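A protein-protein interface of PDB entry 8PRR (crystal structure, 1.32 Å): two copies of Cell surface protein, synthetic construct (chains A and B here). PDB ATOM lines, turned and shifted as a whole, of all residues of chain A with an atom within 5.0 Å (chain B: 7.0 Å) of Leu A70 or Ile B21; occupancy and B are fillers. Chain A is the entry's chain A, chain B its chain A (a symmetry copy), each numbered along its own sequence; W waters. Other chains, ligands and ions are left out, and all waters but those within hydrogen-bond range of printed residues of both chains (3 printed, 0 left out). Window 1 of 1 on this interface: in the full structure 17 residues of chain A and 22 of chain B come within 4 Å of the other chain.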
ATOM      1  N   TYR A  62      24.005  36.875  -1.104  1.00  0.00           N
ATOM      2  CA  TYR A  62      24.495  35.581  -1.549  1.00  0.00           C
ATOM      3  C   TYR A  62      25.385  35.774  -2.768  1.00  0.00           C
ATOM      4  O   TYR A  62      25.055  36.551  -3.667  1.00  0.00           O
ATOM      5  CB  TYR A  62      23.339  34.656  -1.931  1.00  0.00           C
ATOM      6  CG  TYR A  62      22.263  34.536  -0.880  1.00  0.00           C
ATOM      7  CD1 TYR A  62      22.360  33.597   0.137  1.00  0.00           C
ATOM      8  CD2 TYR A  62      21.141  35.352  -0.915  1.00  0.00           C
ATOM      9  CE1 TYR A  62      21.373  33.480   1.096  1.00  0.00           C
ATOM     10  CE2 TYR A  62      20.150  35.242   0.040  1.00  0.00           C
ATOM     11  CZ  TYR A  62      20.271  34.307   1.045  1.00  0.00           C
ATOM     12  OH  TYR A  62      19.283  34.200   1.993  1.00  0.00           O
ATOM     13  N   VAL A  63      26.505  35.059  -2.801  1.00  0.00           N
ATOM     14  CA  VAL A  63      27.432  35.158  -3.922  1.00  0.00           C
ATOM     15  C   VAL A  63      28.281  33.897  -3.957  1.00  0.00           C
ATOM     16  O   VAL A  63      28.664  33.359  -2.915  1.00  0.00           O
ATOM     17  CB  VAL A  63      28.301  36.433  -3.820  1.00  0.00           C
ATOM     18  CG1 VAL A  63      29.368  36.274  -2.738  1.00  0.00           C
ATOM     19  CG2 VAL A  63      28.933  36.751  -5.170  1.00  0.00           C
ATOM     20  N   GLY A  64      28.570  33.427  -5.169  1.00  0.00           N
ATOM     21  CA  GLY A  64      29.481  32.323  -5.343  1.00  0.00           C
ATOM     22  C   GLY A  64      30.931  32.771  -5.389  1.00  0.00           C
ATOM     23  O   GLY A  64      31.241  33.951  -5.551  1.00  0.00           O
ATOM     24  N   HIS A  68      34.673  27.235  -4.714  1.00  0.00           N
ATOM     25  CA  HIS A  68      33.645  26.198  -4.795  1.00  0.00           C
ATOM     26  C   HIS A  68      32.417  26.484  -3.934  1.00  0.00           C
ATOM     27  O   HIS A  68      31.437  25.747  -4.030  1.00  0.00           O
ATOM     28  CB  HIS A  68      34.155  24.777  -4.485  1.00  0.00           C
ATOM     29  CG  HIS A  68      35.323  24.343  -5.313  1.00  0.00           C
ATOM     30  ND1 HIS A  68      35.866  23.081  -5.215  1.00  0.00           N
ATOM     31  CD2 HIS A  68      36.049  24.992  -6.254  1.00  0.00           C
ATOM     32  CE1 HIS A  68      36.878  22.971  -6.057  1.00  0.00           C
ATOM     33  NE2 HIS A  68      37.011  24.118  -6.698  1.00  0.00           N
ATOM     34  N   TYR A  69      32.435  27.514  -3.096  1.00  0.00           N
ATOM     35  CA  TYR A  69      31.362  27.737  -2.142  1.00  0.00           C
ATOM     36  C   TYR A  69      30.383  28.799  -2.631  1.00  0.00           C
ATOM     37  O   TYR A  69      30.757  29.757  -3.313  1.00  0.00           O
ATOM     38  CB  TYR A  69      31.911  28.187  -0.785  1.00  0.00           C
ATOM     39  CG  TYR A  69      32.654  27.126  -0.007  1.00  0.00           C
ATOM     40  CD1 TYR A  69      33.947  26.760  -0.351  1.00  0.00           C
ATOM     41  CD2 TYR A  69      32.064  26.502   1.085  1.00  0.00           C
ATOM     42  CE1 TYR A  69      34.630  25.796   0.367  1.00  0.00           C
ATOM     43  CE2 TYR A  69      32.737  25.540   1.808  1.00  0.00           C
ATOM     44  CZ  TYR A  69      34.019  25.188   1.446  1.00  0.00           C
ATOM     45  OH  TYR A  69      34.689  24.226   2.169  1.00  0.00           O
ATOM     46  N   LEU A  70      29.117  28.608  -2.269  1.00  0.00           N
ATOM     47  CA  LEU A  70      28.133  29.679  -2.261  1.00  0.00           C
ATOM     48  C   LEU A  70      28.124  30.288  -0.865  1.00  0.00           C
ATOM     49  O   LEU A  70      27.962  29.572   0.131  1.00  0.00           O
ATOM     50  CB  LEU A  70      26.742  29.142  -2.592  1.00  0.00           C
ATOM     51  CG  LEU A  70      25.595  30.147  -2.438  1.00  0.00           C
ATOM     52  CD1 LEU A  70      25.708  31.268  -3.460  1.00  0.00           C
ATOM     53  CD2 LEU A  70      24.247  29.455  -2.555  1.00  0.00           C
ATOM     54  N   TYR A  71      28.303  31.602  -0.792  1.00  0.00           N
ATOM     55  CA  TYR A  71      28.376  32.307   0.477  1.00  0.00           C
ATOM     56  C   TYR A  71      27.078  33.052   0.742  1.00  0.00           C
ATOM     57  O   TYR A  71      26.456  33.583  -0.180  1.00  0.00           O
ATOM     58  CB  TYR A  71      29.529  33.312   0.476  1.00  0.00           C
ATOM     59  CG  TYR A  71      30.890  32.685   0.642  1.00  0.00           C
ATOM     60  CD1 TYR A  71      31.577  32.173  -0.447  1.00  0.00           C
ATOM     61  CD2 TYR A  71      31.485  32.597   1.894  1.00  0.00           C
ATOM     62  CE1 TYR A  71      32.821  31.597  -0.300  1.00  0.00           C
ATOM     63  CE2 TYR A  71      32.727  32.022   2.051  1.00  0.00           C
ATOM     64  CZ  TYR A  71      33.392  31.523   0.953  1.00  0.00           C
ATOM     65  OH  TYR A  71      34.633  30.949   1.111  1.00  0.00           O
ATOM     66  N   ALA A  72      26.674  33.078   2.008  1.00  0.00           N
ATOM     67  CA  ALA A  72      25.587  33.921   2.487  1.00  0.00           C
ATOM     68  C   ALA A  72      26.171  34.835   3.552  1.00  0.00           C
ATOM     69  O   ALA A  72      26.631  34.360   4.595  1.00  0.00           O
ATOM     70  CB  ALA A  72      24.453  33.076   3.069  1.00  0.00           C
ATOM     71  N   TRP A  81      26.452  31.680   6.429  1.00  0.00           N
ATOM     72  CA  TRP A  81      26.860  30.304   6.172  1.00  0.00           C
ATOM     73  C   TRP A  81      27.495  30.241   4.790  1.00  0.00           C
ATOM     74  O   TRP A  81      27.391  31.178   3.994  1.00  0.00           O
ATOM     75  CB  TRP A  81      25.691  29.315   6.288  1.00  0.00           C
ATOM     76  CG  TRP A  81      24.453  29.689   5.516  1.00  0.00           C
ATOM     77  CD1 TRP A  81      23.274  30.141   6.034  1.00  0.00           C
ATOM     78  CD2 TRP A  81      24.266  29.623   4.095  1.00  0.00           C
ATOM     79  NE1 TRP A  81      22.370  30.370   5.027  1.00  0.00           N
ATOM     80  CE2 TRP A  81      22.954  30.060   3.827  1.00  0.00           C
ATOM     81  CE3 TRP A  81      25.081  29.241   3.025  1.00  0.00           C
ATOM     82  CZ2 TRP A  81      22.437  30.126   2.534  1.00  0.00           C
ATOM     83  CZ3 TRP A  81      24.568  29.309   1.743  1.00  0.00           C
ATOM     84  CH2 TRP A  81      23.258  29.747   1.508  1.00  0.00           C
ATOM     85  N   LYS A  82      28.162  29.122   4.515  1.00  0.00           N
ATOM     86  CA  LYS A  82      28.712  28.845   3.196  1.00  0.00           C
ATOM     87  C   LYS A  82      28.415  27.395   2.836  1.00  0.00           C
ATOM     88  O   LYS A  82      28.308  26.535   3.715  1.00  0.00           O
ATOM     89  CB  LYS A  82      30.224  29.107   3.131  1.00  0.00           C
ATOM     90  CG  LYS A  82      31.049  28.341   4.153  1.00  0.00           C
ATOM     91  CD  LYS A  82      32.497  28.817   4.152  1.00  0.00           C
ATOM     92  CE  LYS A  82      33.390  27.907   4.981  1.00  0.00           C
ATOM     93  NZ  LYS A  82      34.824  28.036   4.601  1.00  0.00           N
ATOM     94  N   PHE A  83      28.282  27.132   1.536  1.00  0.00           N
ATOM     95  CA  PHE A  83      27.869  25.825   1.038  1.00  0.00           C
ATOM     96  C   PHE A  83      28.825  25.375  -0.058  1.00  0.00           C
ATOM     97  O   PHE A  83      28.951  26.045  -1.085  1.00  0.00           O
ATOM     98  CB  PHE A  83      26.434  25.879   0.503  1.00  0.00           C
ATOM     99  CG  PHE A  83      25.928  24.562  -0.008  1.00  0.00           C
ATOM    100  CD1 PHE A  83      26.180  24.163  -1.311  1.00  0.00           C
ATOM    101  CD2 PHE A  83      25.205  23.719   0.817  1.00  0.00           C
ATOM    102  CE1 PHE A  83      25.718  22.950  -1.780  1.00  0.00           C
ATOM    103  CE2 PHE A  83      24.741  22.505   0.353  1.00  0.00           C
ATOM    104  CZ  PHE A  83      24.998  22.120  -0.946  1.00  0.00           C
ATOM    105  N   THR B   5      30.384  23.342  -3.239  1.00  0.00           N
ATOM    106  CA  THR B   5      29.991  22.477  -4.383  1.00  0.00           C
ATOM    107  C   THR B   5      31.216  21.673  -4.809  1.00  0.00           C
ATOM    108  O   THR B   5      32.248  21.842  -4.180  1.00  0.00           O
ATOM    109  CB  THR B   5      29.414  23.278  -5.568  1.00  0.00           C
ATOM    110  OG1 THR B   5      30.410  24.204  -5.990  1.00  0.00           O
ATOM    111  CG2 THR B   5      28.125  24.004  -5.253  1.00  0.00           C
ATOM    112  N   VAL B   9      31.923  28.352  -8.333  1.00  0.00           N
ATOM    113  CA  VAL B   9      30.574  28.876  -8.454  1.00  0.00           C
ATOM    114  C   VAL B   9      30.671  30.168  -9.263  1.00  0.00           C
ATOM    115  O   VAL B   9      30.707  31.279  -8.711  1.00  0.00           O
ATOM    116  CB  VAL B   9      29.879  29.053  -7.092  1.00  0.00           C
ATOM    117  CG1 VAL B   9      28.443  29.504  -7.284  1.00  0.00           C
ATOM    118  CG2 VAL B   9      29.922  27.743  -6.316  1.00  0.00           C
ATOM    119  N   SER B  11      28.393  30.896 -11.660  1.00  0.00           N
ATOM    120  CA  SER B  11      27.014  31.328 -11.834  1.00  0.00           C
ATOM    121  C   SER B  11      26.599  32.274 -10.713  1.00  0.00           C
ATOM    122  O   SER B  11      27.118  32.217  -9.596  1.00  0.00           O
ATOM    123  CB  SER B  11      26.114  30.085 -11.804  1.00  0.00           C
ATOM    124  OG  SER B  11      24.749  30.402 -11.990  1.00  0.00           O
ATOM    125  N   SER B  12      25.622  33.149 -11.021  1.00  0.00           N
ATOM    126  CA  SER B  12      25.147  34.149 -10.067  1.00  0.00           C
ATOM    127  C   SER B  12      23.822  33.701  -9.473  1.00  0.00           C
ATOM    128  O   SER B  12      22.912  33.329 -10.226  1.00  0.00           O
ATOM    129  CB  SER B  12      24.959  35.484 -10.777  1.00  0.00           C
ATOM    130  OG  SER B  12      26.206  35.986 -11.218  1.00  0.00           O
ATOM    131  N   PRO B  13      23.657  33.728  -8.152  1.00  0.00           N
ATOM    132  CA  PRO B  13      22.448  33.149  -7.556  1.00  0.00           C
ATOM    133  C   PRO B  13      21.181  33.899  -7.931  1.00  0.00           C
ATOM    134  O   PRO B  13      21.185  35.112  -8.164  1.00  0.00           O
ATOM    135  CB  PRO B  13      22.711  33.252  -6.046  1.00  0.00           C
ATOM    136  CG  PRO B  13      23.761  34.313  -5.909  1.00  0.00           C
ATOM    137  CD  PRO B  13      24.620  34.158  -7.122  1.00  0.00           C
ATOM    138  N   ALA B  14      20.087  33.144  -7.998  1.00  0.00           N
ATOM    139  CA  ALA B  14      18.741  33.683  -8.104  1.00  0.00           C
ATOM    140  C   ALA B  14      17.960  33.262  -6.867  1.00  0.00           C
ATOM    141  O   ALA B  14      18.182  32.181  -6.311  1.00  0.00           O
ATOM    142  CB  ALA B  14      18.028  33.162  -9.354  1.00  0.00           C
ATOM    143  N   ILE B  15      17.041  34.121  -6.437  1.00  0.00           N
ATOM    144  CA  ILE B  15      16.318  33.937  -5.183  1.00  0.00           C
ATOM    145  C   ILE B  15      14.840  33.771  -5.501  1.00  0.00           C
ATOM    146  O   ILE B  15      14.235  34.637  -6.144  1.00  0.00           O
ATOM    147  CB  ILE B  15      16.556  35.111  -4.219  1.00  0.00           C
ATOM    148  CG1 ILE B  15      18.056  35.253  -3.943  1.00  0.00           C
ATOM    149  CG2 ILE B  15      15.790  34.899  -2.918  1.00  0.00           C
ATOM    150  CD1 ILE B  15      18.436  36.506  -3.198  1.00  0.00           C
ATOM    151  N   GLY B  16      14.263  32.657  -5.052  1.00  0.00           N
ATOM    152  CA  GLY B  16      12.851  32.418  -5.244  1.00  0.00           C
ATOM    153  C   GLY B  16      12.001  33.176  -4.246  1.00  0.00           C
ATOM    154  O   GLY B  16      12.485  33.738  -3.265  1.00  0.00           O
ATOM    155  N   ASP B  18      10.073  32.130  -2.020  1.00  0.00           N
ATOM    156  CA  ASP B  18      10.147  31.556  -0.683  1.00  0.00           C
ATOM    157  C   ASP B  18      11.551  31.620  -0.089  1.00  0.00           C
ATOM    158  O   ASP B  18      11.775  31.078   0.997  1.00  0.00           O
ATOM    159  CB  ASP B  18       9.630  30.113  -0.690  1.00  0.00           C
ATOM    160  CG  ASP B  18      10.569  29.154  -1.396  1.00  0.00           C
ATOM    161  OD1 ASP B  18      11.483  29.620  -2.106  1.00  0.00           O
ATOM    162  OD2 ASP B  18      10.388  27.926  -1.236  1.00  0.00           O
ATOM    163  N   GLY B  19      12.493  32.270  -0.770  1.00  0.00           N
ATOM    164  CA  GLY B  19      13.837  32.444  -0.264  1.00  0.00           C
ATOM    165  C   GLY B  19      14.843  31.427  -0.758  1.00  0.00           C
ATOM    166  O   GLY B  19      16.041  31.587  -0.486  1.00  0.00           O
ATOM    167  N   THR B  20      14.399  30.389  -1.463  1.00  0.00           N
ATOM    168  CA  THR B  20      15.326  29.405  -2.002  1.00  0.00           C
ATOM    169  C   THR B  20      16.344  30.086  -2.905  1.00  0.00           C
ATOM    170  O   THR B  20      15.996  30.932  -3.733  1.00  0.00           O
ATOM    171  CB  THR B  20      14.553  28.355  -2.803  1.00  0.00           C
ATOM    172  OG1 THR B  20      13.541  27.764  -1.977  1.00  0.00           O
ATOM    173  CG2 THR B  20      15.492  27.267  -3.309  1.00  0.00           C
ATOM    174  N   ILE B  21      17.609  29.716  -2.741  1.00  0.00           N
ATOM    175  CA  ILE B  21      18.702  30.268  -3.532  1.00  0.00           C
ATOM    176  C   ILE B  21      19.104  29.235  -4.575  1.00  0.00           C
ATOM    177  O   ILE B  21      19.455  28.099  -4.234  1.00  0.00           O
ATOM    178  CB  ILE B  21      19.894  30.657  -2.644  1.00  0.00           C
ATOM    179  CG1 ILE B  21      19.434  31.594  -1.528  1.00  0.00           C
ATOM    180  CG2 ILE B  21      20.980  31.320  -3.481  1.00  0.00           C
ATOM    181  CD1 ILE B  21      19.227  30.901  -0.196  1.00  0.00           C
ATOM    182  N   TYR B  22      19.048  29.623  -5.845  1.00  0.00           N
ATOM    183  CA  TYR B  22      19.418  28.755  -6.955  1.00  0.00           C
ATOM    184  C   TYR B  22      20.702  29.276  -7.579  1.00  0.00           C
ATOM    185  O   TYR B  22      20.817  30.474  -7.855  1.00  0.00           O
ATOM    186  CB  TYR B  22      18.320  28.740  -8.019  1.00  0.00           C
ATOM    187  CG  TYR B  22      16.945  28.394  -7.500  1.00  0.00           C
ATOM    188  CD1 TYR B  22      16.549  27.072  -7.359  1.00  0.00           C
ATOM    189  CD2 TYR B  22      16.035  29.389  -7.172  1.00  0.00           C
ATOM    190  CE1 TYR B  22      15.290  26.751  -6.892  1.00  0.00           C
ATOM    191  CE2 TYR B  22      14.774  29.078  -6.707  1.00  0.00           C
ATOM    192  CZ  TYR B  22      14.406  27.758  -6.570  1.00  0.00           C
ATOM    193  OH  TYR B  22      13.148  27.446  -6.108  1.00  0.00           O
ATOM    194  N   VAL B  23      21.659  28.384  -7.812  1.00  0.00           N
ATOM    195  CA  VAL B  23      22.932  28.783  -8.404  1.00  0.00           C
ATOM    196  C   VAL B  23      23.552  27.574  -9.087  1.00  0.00           C
ATOM    197  O   VAL B  23      23.417  26.439  -8.621  1.00  0.00           O
ATOM    198  CB  VAL B  23      23.875  29.403  -7.343  1.00  0.00           C
ATOM    199  CG1 VAL B  23      24.517  28.321  -6.483  1.00  0.00           C
ATOM    200  CG2 VAL B  23      24.937  30.255  -8.018  1.00  0.00           C
ATOM    201  N   TYR B  31      22.112  24.041  -8.229  1.00  0.00           N
ATOM    202  CA  TYR B  31      21.849  23.824  -6.816  1.00  0.00           C
ATOM    203  C   TYR B  31      20.647  24.644  -6.374  1.00  0.00           C
ATOM    204  O   TYR B  31      20.446  25.769  -6.838  1.00  0.00           O
ATOM    205  CB  TYR B  31      23.068  24.215  -5.975  1.00  0.00           C
ATOM    206  CG  TYR B  31      24.182  23.201  -6.030  1.00  0.00           C
ATOM    207  CD1 TYR B  31      25.136  23.239  -7.038  1.00  0.00           C
ATOM    208  CD2 TYR B  31      24.275  22.195  -5.080  1.00  0.00           C
ATOM    209  CE1 TYR B  31      26.152  22.307  -7.094  1.00  0.00           C
ATOM    210  CE2 TYR B  31      25.287  21.259  -5.125  1.00  0.00           C
ATOM    211  CZ  TYR B  31      26.223  21.318  -6.135  1.00  0.00           C
ATOM    212  OH  TYR B  31      27.233  20.385  -6.181  1.00  0.00           O
ATOM    213  N   ALA B  32      19.848  24.063  -5.484  1.00  0.00           N
ATOM    214  CA  ALA B  32      18.739  24.743  -4.824  1.00  0.00           C
ATOM    215  C   ALA B  32      18.993  24.627  -3.327  1.00  0.00           C
ATOM    216  O   ALA B  32      18.936  23.527  -2.767  1.00  0.00           O
ATOM    217  CB  ALA B  32      17.404  24.106  -5.199  1.00  0.00           C
ATOM    218  N   ILE B  33      19.283  25.754  -2.684  1.00  0.00           N
ATOM    219  CA  ILE B  33      19.728  25.781  -1.297  1.00  0.00           C
ATOM    220  C   ILE B  33      18.721  26.582  -0.487  1.00  0.00           C
ATOM    221  O   ILE B  33      18.283  27.656  -0.916  1.00  0.00           O
ATOM    222  CB  ILE B  33      21.145  26.374  -1.186  1.00  0.00           C
ATOM    223  CG1 ILE B  33      22.129  25.514  -1.988  1.00  0.00           C
ATOM    224  CG2 ILE B  33      21.589  26.450   0.267  1.00  0.00           C
ATOM    225  CD1 ILE B  33      23.418  26.211  -2.337  1.00  0.00           C
ATOM    226  N   ASN B  34      18.348  26.054   0.674  1.00  0.00           N
ATOM    227  CA  ASN B  34      17.392  26.722   1.540  1.00  0.00           C
ATOM    228  C   ASN B  34      18.054  27.901   2.245  1.00  0.00           C
ATOM    229  O   ASN B  34      19.278  27.942   2.393  1.00  0.00           O
ATOM    230  CB  ASN B  34      16.864  25.740   2.581  1.00  0.00           C
ATOM    231  CG  ASN B  34      16.028  24.634   1.967  1.00  0.00           C
ATOM    232  OD1 ASN B  34      15.110  24.893   1.190  1.00  0.00           O
ATOM    233  ND2 ASN B  34      16.342  23.391   2.317  1.00  0.00           N
ATOM    234  N   PRO B  35      17.263  28.879   2.693  1.00  0.00           N
ATOM    235  CA  PRO B  35      17.856  30.052   3.358  1.00  0.00           C
ATOM    236  C   PRO B  35      18.721  29.712   4.558  1.00  0.00           C
ATOM    237  O   PRO B  35      19.579  30.523   4.928  1.00  0.00           O
ATOM    238  CB  PRO B  35      16.631  30.887   3.759  1.00  0.00           C
ATOM    239  CG  PRO B  35      15.581  30.490   2.776  1.00  0.00           C
ATOM    240  CD  PRO B  35      15.802  29.019   2.546  1.00  0.00           C
ATOM    241  N   ASN B  36      18.523  28.551   5.183  1.00  0.00           N
ATOM    242  CA  ASN B  36      19.355  28.145   6.310  1.00  0.00           C
ATOM    243  C   ASN B  36      20.678  27.526   5.876  1.00  0.00           C
ATOM    244  O   ASN B  36      21.457  27.103   6.737  1.00  0.00           O
ATOM    245  CB  ASN B  36      18.610  27.153   7.213  1.00  0.00           C
ATOM    246  CG  ASN B  36      18.098  25.943   6.457  1.00  0.00           C
ATOM    247  OD1 ASN B  36      18.618  25.589   5.398  1.00  0.00           O
ATOM    248  ND2 ASN B  36      17.086  25.284   7.014  1.00  0.00           N
ATOM    249  N   GLY B  37      20.944  27.449   4.573  1.00  0.00           N
ATOM    250  CA  GLY B  37      22.186  26.903   4.074  1.00  0.00           C
ATOM    251  C   GLY B  37      22.179  25.414   3.815  1.00  0.00           C
ATOM    252  O   GLY B  37      23.224  24.865   3.443  1.00  0.00           O
ATOM    253  N   LYS B  40      18.444  21.848  -0.700  1.00  0.00           N
ATOM    254  CA  LYS B  40      17.104  21.386  -1.039  1.00  0.00           C
ATOM    255  C   LYS B  40      17.159  20.310  -2.121  1.00  0.00           C
ATOM    256  O   LYS B  40      16.612  19.218  -1.942  1.00  0.00           O
ATOM    257  CB  LYS B  40      16.224  22.560  -1.478  1.00  0.00           C
ATOM    258  CG  LYS B  40      14.744  22.205  -1.607  1.00  0.00           C
ATOM    259  CD  LYS B  40      13.977  23.225  -2.448  1.00  0.00           C
ATOM    260  CE  LYS B  40      13.409  24.392  -1.632  1.00  0.00           C
ATOM    261  NZ  LYS B  40      13.107  24.086  -0.204  1.00  0.00           N
ATOM    262  N   TRP B  41      17.818  20.600  -3.241  1.00  0.00           N
ATOM    263  CA  TRP B  41      18.107  19.578  -4.236  1.00  0.00           C
ATOM    264  C   TRP B  41      19.208  20.091  -5.155  1.00  0.00           C
ATOM    265  O   TRP B  41      19.578  21.267  -5.122  1.00  0.00           O
ATOM    266  CB  TRP B  41      16.868  19.190  -5.053  1.00  0.00           C
ATOM    267  CG  TRP B  41      16.061  20.348  -5.574  1.00  0.00           C
ATOM    268  CD1 TRP B  41      14.884  20.818  -5.067  1.00  0.00           C
ATOM    269  CD2 TRP B  41      16.364  21.171  -6.709  1.00  0.00           C
ATOM    270  NE1 TRP B  41      14.437  21.880  -5.815  1.00  0.00           N
ATOM    271  CE2 TRP B  41      15.328  22.118  -6.827  1.00  0.00           C
ATOM    272  CE3 TRP B  41      17.412  21.197  -7.636  1.00  0.00           C
ATOM    273  CZ2 TRP B  41      15.309  23.082  -7.834  1.00  0.00           C
ATOM    274  CZ3 TRP B  41      17.390  22.157  -8.635  1.00  0.00           C
ATOM    275  CH2 TRP B  41      16.346  23.085  -8.725  1.00  0.00           C
ATOM    276  N   PRO B  53      20.767  31.363 -13.144  1.00  0.00           N
ATOM    277  CA  PRO B  53      19.371  30.959 -13.339  1.00  0.00           C
ATOM    278  C   PRO B  53      18.406  32.132 -13.299  1.00  0.00           C
ATOM    279  O   PRO B  53      18.643  33.150 -12.642  1.00  0.00           O
ATOM    280  CB  PRO B  53      19.113  29.997 -12.173  1.00  0.00           C
ATOM    281  CG  PRO B  53      20.114  30.373 -11.133  1.00  0.00           C
ATOM    282  CD  PRO B  53      21.321  30.869 -11.869  1.00  0.00           C
HETATM  283  O   HOH W   1      16.757  33.828   0.718  1.00  0.00           O
HETATM  284  O   HOH W   2      19.826  33.143   4.258  1.00  0.00           O
HETATM  285  O   HOH W   3      25.636  25.585   4.760  1.00  0.00           O
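Water W2 lies within hydrogen-bond range of the side-chain hydroxyl of Tyr A62 and the backbone carbonyl oxygen of Pro B35.
Water W1 bridges the backbone carbonyl oxygen of Gly B19 (2.6 Å) and the side-chain hydroxyl of Tyr A62 (2.9 Å).
Water W3 bridges the backbone carbonyl oxygen (O) of Gly B37 and the backbone carbonyl oxygen (O) of Lys A82.
No position is printed for both chains.
Of the 18 pairs that touch across the chains among the printed residues, none has its exchanged pair printed and touching as well.
Of the 11 printed residues of chain A, 7 touch a printed residue of chain B.
Hydrophobic or aromatic side chains of chain A within 4 Å of the printed part of chain B: Tyr A62, His A68, Leu A70, Trp A81 and Phe A83.
Along chain A the printed residues that touch a printed residue of chain B span positions 62 to 83.
Of the printed residues of chain B, Tyr A62 touches Pro B13, Ile B15 and Ile B21.
Leu A70 touches two residues of chain B.
Printed residues of chain A within 4 Å of Val B9: Gly A64, His A68 and Tyr A69.
Printed residues of chain A within 4 Å of Pro B13: Tyr A62 (3.4 Å).
Printed residues of chain A within 4 Å of Ile B15: Tyr A62 (3.7 Å).
Ile B21 touches two residues of chain A.
Of the printed residues of chain A, Ile B33 touches Leu A70, Trp A81 and Phe A83.
The nearest residue of chain A that does not touch Ile B21 is Trp A81 (4.3 Å).
The nearest printed residue of chain A that does not touch Pro B13 is Val A63 (4.2 Å).
Among the printed residues, pairs that only touch across the chains: Tyr A62 with Pro B13 (3.4 Å), Tyr A62 with Ile B15 (3.7 Å), Tyr A62 with Ile B21 (3.6 Å), Gly A64 with Val B9 (3.6 Å), His A68 with Val B9 (3.4 Å), Tyr A69 with Val B9 (3.7 Å), Leu A70 with Ile B21 (3.9 Å), Leu A70 with Ile B33 (3.4 Å), Trp A81 with Ile B33 (3.9 Å), Trp A81 with Asn B34 (3.8 Å), Trp A81 with Asn B36 (3.4 Å), Phe A83 with Thr B5 (3.7 Å), Phe A83 with Tyr B31 (3.7 Å), Phe A83 with Ile B33 (3.6 Å) and Phe A83 with Gly B37 (3.5 Å).
N of Leu A70 sits at hydrogen-bond distance from O of Phe A83.
The backbone NH (N) of Ala A72 sits at hydrogen-bond distance from the backbone carbonyl oxygen (O) of Trp A81 (2.8 Å).
O of Ile B21 lies within hydrogen-bond range of N of Ile B33 (2.8 Å).
O of Val B23 lies within hydrogen-bond range of N of Tyr B31, 2.8 Å away.
OD1 of Asn B34 lies within hydrogen-bond range of NZ of Lys B40 (2.6 Å).
The side-chain hydroxyl (OG1) of Thr B5 lies within hydrogen-bond range of the backbone carbonyl oxygen (O) of His A68 (2.7 Å).
The backbone carbonyl oxygen (O) of Pro B35 sits at hydrogen-bond distance from the indole nitrogen (NE1) of Trp A81 (2.8 Å).
NE1 of Trp A81 lies close to N of Gly B37.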
